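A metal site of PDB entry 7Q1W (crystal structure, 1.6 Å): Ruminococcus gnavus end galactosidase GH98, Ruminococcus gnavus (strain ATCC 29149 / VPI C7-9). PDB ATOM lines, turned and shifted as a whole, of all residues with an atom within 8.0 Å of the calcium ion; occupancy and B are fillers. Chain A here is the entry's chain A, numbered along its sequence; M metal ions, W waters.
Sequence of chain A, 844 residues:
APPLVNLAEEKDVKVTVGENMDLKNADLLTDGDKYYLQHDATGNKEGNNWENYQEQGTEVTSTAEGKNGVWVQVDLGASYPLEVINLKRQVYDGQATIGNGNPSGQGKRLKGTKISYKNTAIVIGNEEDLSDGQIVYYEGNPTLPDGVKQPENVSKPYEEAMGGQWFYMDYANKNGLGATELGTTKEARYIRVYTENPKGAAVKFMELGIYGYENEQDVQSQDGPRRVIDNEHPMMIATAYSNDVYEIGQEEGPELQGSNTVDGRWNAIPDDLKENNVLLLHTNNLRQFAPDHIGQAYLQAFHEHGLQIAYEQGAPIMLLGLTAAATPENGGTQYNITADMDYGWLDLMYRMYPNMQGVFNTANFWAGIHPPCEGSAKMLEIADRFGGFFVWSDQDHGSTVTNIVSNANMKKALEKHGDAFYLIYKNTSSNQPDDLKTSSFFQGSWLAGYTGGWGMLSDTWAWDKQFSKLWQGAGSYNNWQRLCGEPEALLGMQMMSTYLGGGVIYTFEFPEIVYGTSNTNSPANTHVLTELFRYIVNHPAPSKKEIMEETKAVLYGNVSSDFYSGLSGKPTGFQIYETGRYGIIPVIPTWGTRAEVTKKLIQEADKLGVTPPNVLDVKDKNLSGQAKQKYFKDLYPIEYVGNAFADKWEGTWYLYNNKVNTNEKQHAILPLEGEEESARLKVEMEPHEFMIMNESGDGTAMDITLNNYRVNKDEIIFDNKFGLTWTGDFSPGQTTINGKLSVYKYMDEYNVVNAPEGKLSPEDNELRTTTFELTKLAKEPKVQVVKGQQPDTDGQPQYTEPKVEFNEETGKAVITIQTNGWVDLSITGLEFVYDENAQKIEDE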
ATOM      1  N   HIS A 527     -15.832  15.578 -31.686  1.00  0.00           N
ATOM      2  CA  HIS A 527     -16.551  15.367 -30.401  1.00  0.00           C
ATOM      3  C   HIS A 527     -17.857  14.612 -30.587  1.00  0.00           C
ATOM      4  O   HIS A 527     -18.381  14.173 -29.575  1.00  0.00           O
ATOM      5  CB  HIS A 527     -16.754  16.714 -29.699  1.00  0.00           C
ATOM      6  CG  HIS A 527     -15.450  17.354 -29.348  1.00  0.00           C
ATOM      7  ND1 HIS A 527     -14.465  16.662 -28.695  1.00  0.00           N
ATOM      8  CD2 HIS A 527     -14.977  18.606 -29.552  1.00  0.00           C
ATOM      9  CE1 HIS A 527     -13.436  17.484 -28.472  1.00  0.00           C
ATOM     10  NE2 HIS A 527     -13.733  18.683 -28.982  1.00  0.00           N
ATOM     11  N   TYR A 709     -22.843  17.664 -27.079  1.00  0.00           N
ATOM     12  CA  TYR A 709     -21.937  18.694 -27.599  1.00  0.00           C
ATOM     13  C   TYR A 709     -22.695  19.714 -28.470  1.00  0.00           C
ATOM     14  O   TYR A 709     -23.322  19.326 -29.456  1.00  0.00           O
ATOM     15  CB  TYR A 709     -20.861  18.057 -28.481  1.00  0.00           C
ATOM     16  CG  TYR A 709     -19.752  19.008 -28.776  1.00  0.00           C
ATOM     17  CD1 TYR A 709     -18.967  19.531 -27.761  1.00  0.00           C
ATOM     18  CD2 TYR A 709     -19.484  19.403 -30.077  1.00  0.00           C
ATOM     19  CE1 TYR A 709     -17.963  20.439 -28.027  1.00  0.00           C
ATOM     20  CE2 TYR A 709     -18.470  20.304 -30.351  1.00  0.00           C
ATOM     21  CZ  TYR A 709     -17.708  20.836 -29.332  1.00  0.00           C
ATOM     22  OH  TYR A 709     -16.734  21.742 -29.648  1.00  0.00           O
ATOM     23  N   SER A 761     -10.482  28.458 -29.527  1.00  0.00           N
ATOM     24  CA  SER A 761     -11.168  27.226 -29.090  1.00  0.00           C
ATOM     25  C   SER A 761     -12.656  27.387 -29.390  1.00  0.00           C
ATOM     26  O   SER A 761     -13.183  28.504 -29.331  1.00  0.00           O
ATOM     27  CB  SER A 761     -11.000  27.006 -27.588  1.00  0.00           C
ATOM     28  OG  SER A 761      -9.631  26.799 -27.231  1.00  0.00           O
ATOM     29  N   PRO A 762     -13.392  26.276 -29.566  1.00  0.00           N
ATOM     30  CA  PRO A 762     -14.819  26.342 -29.864  1.00  0.00           C
ATOM     31  C   PRO A 762     -15.595  26.915 -28.682  1.00  0.00           C
ATOM     32  O   PRO A 762     -15.230  26.711 -27.515  1.00  0.00           O
ATOM     33  CB  PRO A 762     -15.206  24.890 -30.190  1.00  0.00           C
ATOM     34  CG  PRO A 762     -13.863  24.206 -30.441  1.00  0.00           C
ATOM     35  CD  PRO A 762     -12.936  24.877 -29.444  1.00  0.00           C
ATOM     36  N   GLU A 763     -16.633  27.704 -29.004  1.00  0.00           N
ATOM     37  CA  GLU A 763     -17.569  28.259 -27.996  1.00  0.00           C
ATOM     38  C   GLU A 763     -18.532  27.179 -27.518  1.00  0.00           C
ATOM     39  O   GLU A 763     -19.726  27.238 -27.838  1.00  0.00           O
ATOM     40  CB  GLU A 763     -18.331  29.449 -28.573  1.00  0.00           C
ATOM     41  CG  GLU A 763     -17.471  30.678 -28.634  1.00  0.00           C
ATOM     42  CD  GLU A 763     -17.144  31.299 -27.278  1.00  0.00           C
ATOM     43  OE1 GLU A 763     -17.682  30.855 -26.239  1.00  0.00           O
ATOM     44  OE2 GLU A 763     -16.339  32.237 -27.277  1.00  0.00           O
ATOM     45  N   ASP A 764     -18.032  26.277 -26.681  1.00  0.00           N
ATOM     46  CA  ASP A 764     -18.761  25.052 -26.276  1.00  0.00           C
ATOM     47  C   ASP A 764     -18.721  24.905 -24.751  1.00  0.00           C
ATOM     48  O   ASP A 764     -18.873  23.742 -24.255  1.00  0.00           O
ATOM     49  CB  ASP A 764     -18.145  23.802 -26.923  1.00  0.00           C
ATOM     50  CG  ASP A 764     -16.676  23.643 -26.606  1.00  0.00           C
ATOM     51  OD1 ASP A 764     -16.261  24.263 -25.590  1.00  0.00           O
ATOM     52  OD2 ASP A 764     -15.970  22.905 -27.367  1.00  0.00           O
ATOM     53  N   ASN A 765     -18.501  26.004 -24.023  1.00  0.00           N
ATOM     54  CA  ASN A 765     -18.199  25.959 -22.564  1.00  0.00           C
ATOM     55  C   ASN A 765     -19.462  26.156 -21.723  1.00  0.00           C
ATOM     56  O   ASN A 765     -19.361  26.022 -20.464  1.00  0.00           O
ATOM     57  CB  ASN A 765     -17.135  26.987 -22.225  1.00  0.00           C
ATOM     58  CG  ASN A 765     -15.858  26.635 -22.946  1.00  0.00           C
ATOM     59  OD1 ASN A 765     -15.557  25.460 -23.069  1.00  0.00           O
ATOM     60  ND2 ASN A 765     -15.129  27.627 -23.435  1.00  0.00           N
ATOM     61  N   GLU A 766     -20.604  26.505 -22.324  1.00  0.00           N
ATOM     62  CA  GLU A 766     -21.853  26.683 -21.540  1.00  0.00           C
ATOM     63  C   GLU A 766     -22.455  25.297 -21.306  1.00  0.00           C
ATOM     64  O   GLU A 766     -22.814  24.626 -22.293  1.00  0.00           O
ATOM     65  CB  GLU A 766     -22.860  27.608 -22.219  1.00  0.00           C
ATOM     66  CG  GLU A 766     -24.044  27.942 -21.297  1.00  0.00           C
ATOM     67  CD  GLU A 766     -25.226  28.727 -21.883  1.00  0.00           C
ATOM     68  OE1 GLU A 766     -25.047  29.374 -22.918  1.00  0.00           O
ATOM     69  OE2 GLU A 766     -26.313  28.721 -21.270  1.00  0.00           O
ATOM     70  N   LEU A 767     -22.568  24.876 -20.046  1.00  0.00           N
ATOM     71  CA  LEU A 767     -22.956  23.484 -19.736  1.00  0.00           C
ATOM     72  C   LEU A 767     -24.472  23.373 -19.512  1.00  0.00           C
ATOM     73  O   LEU A 767     -25.140  24.353 -19.094  1.00  0.00           O
ATOM     74  CB  LEU A 767     -22.190  22.979 -18.523  1.00  0.00           C
ATOM     75  CG  LEU A 767     -20.685  23.221 -18.522  1.00  0.00           C
ATOM     76  CD1 LEU A 767     -20.108  22.625 -17.236  1.00  0.00           C
ATOM     77  CD2 LEU A 767     -20.030  22.628 -19.774  1.00  0.00           C
ATOM     78  N   GLN A 789     -14.896  14.161 -21.880  1.00  0.00           N
ATOM     79  CA  GLN A 789     -14.282  15.120 -22.810  1.00  0.00           C
ATOM     80  C   GLN A 789     -13.495  16.171 -22.046  1.00  0.00           C
ATOM     81  O   GLN A 789     -14.017  16.731 -21.057  1.00  0.00           O
ATOM     82  CB  GLN A 789     -15.368  15.776 -23.640  1.00  0.00           C
ATOM     83  CG  GLN A 789     -14.806  16.594 -24.779  1.00  0.00           C
ATOM     84  CD  GLN A 789     -15.926  17.138 -25.609  1.00  0.00           C
ATOM     85  OE1 GLN A 789     -16.948  16.466 -25.812  1.00  0.00           O
ATOM     86  NE2 GLN A 789     -15.749  18.358 -26.082  1.00  0.00           N
ATOM     87  N   GLN A 790     -12.240  16.370 -22.437  1.00  0.00           N
ATOM     88  CA  GLN A 790     -11.330  17.284 -21.713  1.00  0.00           C
ATOM     89  C   GLN A 790     -11.401  18.667 -22.367  1.00  0.00           C
ATOM     90  O   GLN A 790     -11.952  18.836 -23.465  1.00  0.00           O
ATOM     91  CB  GLN A 790      -9.921  16.657 -21.620  1.00  0.00           C
ATOM     92  CG  GLN A 790      -9.825  15.434 -20.704  1.00  0.00           C
ATOM     93  CD  GLN A 790     -10.270  15.688 -19.286  1.00  0.00           C
ATOM     94  OE1 GLN A 790      -9.724  16.535 -18.577  1.00  0.00           O
ATOM     95  NE2 GLN A 790     -11.292  14.970 -18.843  1.00  0.00           N
ATOM     96  N   PRO A 791     -10.933  19.711 -21.643  1.00  0.00           N
ATOM     97  CA  PRO A 791     -10.907  21.070 -22.167  1.00  0.00           C
ATOM     98  C   PRO A 791     -10.177  21.205 -23.505  1.00  0.00           C
ATOM     99  O   PRO A 791      -9.323  20.397 -23.859  1.00  0.00           O
ATOM    100  CB  PRO A 791     -10.231  21.882 -21.060  1.00  0.00           C
ATOM    101  CG  PRO A 791     -10.566  21.096 -19.804  1.00  0.00           C
ATOM    102  CD  PRO A 791     -10.456  19.653 -20.243  1.00  0.00           C
ATOM    103  N   ASP A 792     -10.588  22.230 -24.246  1.00  0.00           N
ATOM    104  CA  ASP A 792      -9.754  22.797 -25.335  1.00  0.00           C
ATOM    105  C   ASP A 792      -8.633  23.598 -24.651  1.00  0.00           C
ATOM    106  O   ASP A 792      -8.516  23.540 -23.415  1.00  0.00           O
ATOM    107  CB  ASP A 792     -10.592  23.651 -26.285  1.00  0.00           C
ATOM    108  CG  ASP A 792     -10.088  23.543 -27.711  1.00  0.00           C
ATOM    109  OD1 ASP A 792     -10.527  22.607 -28.395  1.00  0.00           O
ATOM    110  OD2 ASP A 792      -9.206  24.317 -28.059  1.00  0.00           O
ATOM    111  N   THR A 793      -7.849  24.324 -25.445  1.00  0.00           N
ATOM    112  CA  THR A 793      -6.642  25.047 -24.992  1.00  0.00           C
ATOM    113  C   THR A 793      -7.039  26.250 -24.150  1.00  0.00           C
ATOM    114  O   THR A 793      -6.158  26.784 -23.505  1.00  0.00           O
ATOM    115  CB  THR A 793      -5.784  25.419 -26.203  1.00  0.00           C
ATOM    116  OG1 THR A 793      -6.626  26.098 -27.128  1.00  0.00           O
ATOM    117  CG2 THR A 793      -5.123  24.204 -26.821  1.00  0.00           C
ATOM    118  N   ASP A 794      -8.308  26.630 -24.114  1.00  0.00           N
ATOM    119  CA  ASP A 794      -8.830  27.694 -23.230  1.00  0.00           C
ATOM    120  C   ASP A 794      -8.995  27.190 -21.779  1.00  0.00           C
ATOM    121  O   ASP A 794      -9.378  27.995 -20.931  1.00  0.00           O
ATOM    122  CB  ASP A 794     -10.124  28.272 -23.807  1.00  0.00           C
ATOM    123  CG  ASP A 794     -11.306  27.324 -23.820  1.00  0.00           C
ATOM    124  OD1 ASP A 794     -11.185  26.210 -23.238  1.00  0.00           O
ATOM    125  OD2 ASP A 794     -12.335  27.702 -24.426  1.00  0.00           O
ATOM    126  N   GLY A 795      -8.789  25.899 -21.522  1.00  0.00           N
ATOM    127  CA  GLY A 795      -8.804  25.301 -20.181  1.00  0.00           C
ATOM    128  C   GLY A 795     -10.181  25.190 -19.560  1.00  0.00           C
ATOM    129  O   GLY A 795     -10.278  24.783 -18.389  1.00  0.00           O
ATOM    130  N   GLN A 796     -11.249  25.541 -20.277  1.00  0.00           N
ATOM    131  CA  GLN A 796     -12.601  25.497 -19.686  1.00  0.00           C
ATOM    132  C   GLN A 796     -13.120  24.049 -19.757  1.00  0.00           C
ATOM    133  O   GLN A 796     -12.980  23.357 -20.780  1.00  0.00           O
ATOM    134  CB  GLN A 796     -13.489  26.506 -20.393  1.00  0.00           C
ATOM    135  CG  GLN A 796     -12.964  27.924 -20.349  1.00  0.00           C
ATOM    136  CD  GLN A 796     -12.930  28.402 -18.921  1.00  0.00           C
ATOM    137  OE1 GLN A 796     -13.813  28.087 -18.115  1.00  0.00           O
ATOM    138  NE2 GLN A 796     -11.884  29.125 -18.581  1.00  0.00           N
ATOM    139  N   PRO A 797     -13.744  23.571 -18.674  1.00  0.00           N
ATOM    140  CA  PRO A 797     -14.250  22.212 -18.583  1.00  0.00           C
ATOM    141  C   PRO A 797     -15.528  21.983 -19.408  1.00  0.00           C
ATOM    142  O   PRO A 797     -16.353  22.915 -19.574  1.00  0.00           O
ATOM    143  CB  PRO A 797     -14.541  22.052 -17.080  1.00  0.00           C
ATOM    144  CG  PRO A 797     -14.909  23.444 -16.641  1.00  0.00           C
ATOM    145  CD  PRO A 797     -13.976  24.338 -17.452  1.00  0.00           C
ATOM    146  N   GLN A 798     -15.680  20.750 -19.879  1.00  0.00           N
ATOM    147  CA  GLN A 798     -16.830  20.282 -20.692  1.00  0.00           C
ATOM    148  C   GLN A 798     -17.806  19.523 -19.810  1.00  0.00           C
ATOM    149  O   GLN A 798     -18.879  19.131 -20.289  1.00  0.00           O
ATOM    150  CB  GLN A 798     -16.323  19.467 -21.881  1.00  0.00           C
ATOM    151  CG  GLN A 798     -15.318  20.219 -22.735  1.00  0.00           C
ATOM    152  CD  GLN A 798     -15.775  21.570 -23.226  1.00  0.00           C
ATOM    153  OE1 GLN A 798     -14.979  22.499 -23.361  1.00  0.00           O
ATOM    154  NE2 GLN A 798     -17.042  21.672 -23.600  1.00  0.00           N
ATOM    155  N   ASN A 820     -21.221  19.748 -21.665  1.00  0.00           N
ATOM    156  CA  ASN A 820     -21.310  20.161 -23.080  1.00  0.00           C
ATOM    157  C   ASN A 820     -20.260  19.336 -23.828  1.00  0.00           C
ATOM    158  O   ASN A 820     -19.094  19.732 -23.906  1.00  0.00           O
ATOM    159  CB  ASN A 820     -21.110  21.656 -23.270  1.00  0.00           C
ATOM    160  CG  ASN A 820     -21.473  22.049 -24.671  1.00  0.00           C
ATOM    161  OD1 ASN A 820     -21.304  21.249 -25.595  1.00  0.00           O
ATOM    162  ND2 ASN A 820     -21.930  23.281 -24.841  1.00  0.00           N
HETATM  163 CA    CA M   1     -14.478  24.128 -24.419  1.00  0.00          CA
HETATM  164  O   HOH W   1     -13.786  22.625 -25.957  1.00  0.00           O
HETATM  165  O   HOH W   2     -13.650  25.679 -25.645  1.00  0.00           O
HETATM  166  O   HOH W   3     -12.670  24.137 -23.212  1.00  0.00           O
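OE1 of Gln 798 is bound to the calcium ion, 2.0 Å away.
OD1 of Asp 764 is bound to the calcium ion (2.1 Å).
The calcium ion is bound by water W2 (2.1 Å).
Water W3 is bound to the calcium ion, at 2.2 Å.
OD1 of Asn 765 is bound to the calcium ion, 2.2 Å away.
The calcium ion is bound by water W1 (2.3 Å).
Water W3 lies within hydrogen-bond range of the side-chain carboxylate (OD1) of Asp 794 (2.6 Å), the backbone carbonyl oxygen (O) of Gln 796 (2.6 Å) and the backbone NH (N) of Asp 792 (3.0 Å).
Water W2 lies within hydrogen-bond range of O of Pro 762 (2.7 Å), OD2 of Asp 794 (2.7 Å) and ND2 of Asn 765 (3.3 Å).
The side-chain amide oxygen (OE1) of Gln 798 lies close to the backbone carbonyl oxygen (O) of Gln 796.
The side-chain hydroxyl of Tyr 709 lies within hydrogen-bond range of the side-chain carboxylate of Asp 764.
O of Asp 764 sits close to ND2 of Asn 820 (3.1 Å).
ND2 of Asn 765 lies within hydrogen-bond range of OD2 of Asp 794 (3.0 Å).
The backbone carbonyl oxygen of Gln 798 is in hydrogen-bond range of the backbone NH of Asn 820, at 2.8 Å.
Within 4 Å of the calcium ion: Asp 764, Asn 765 and Gln 798.
The nearest printed residue that does not touch the calcium ion is Gln 796 (4.01 Å).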
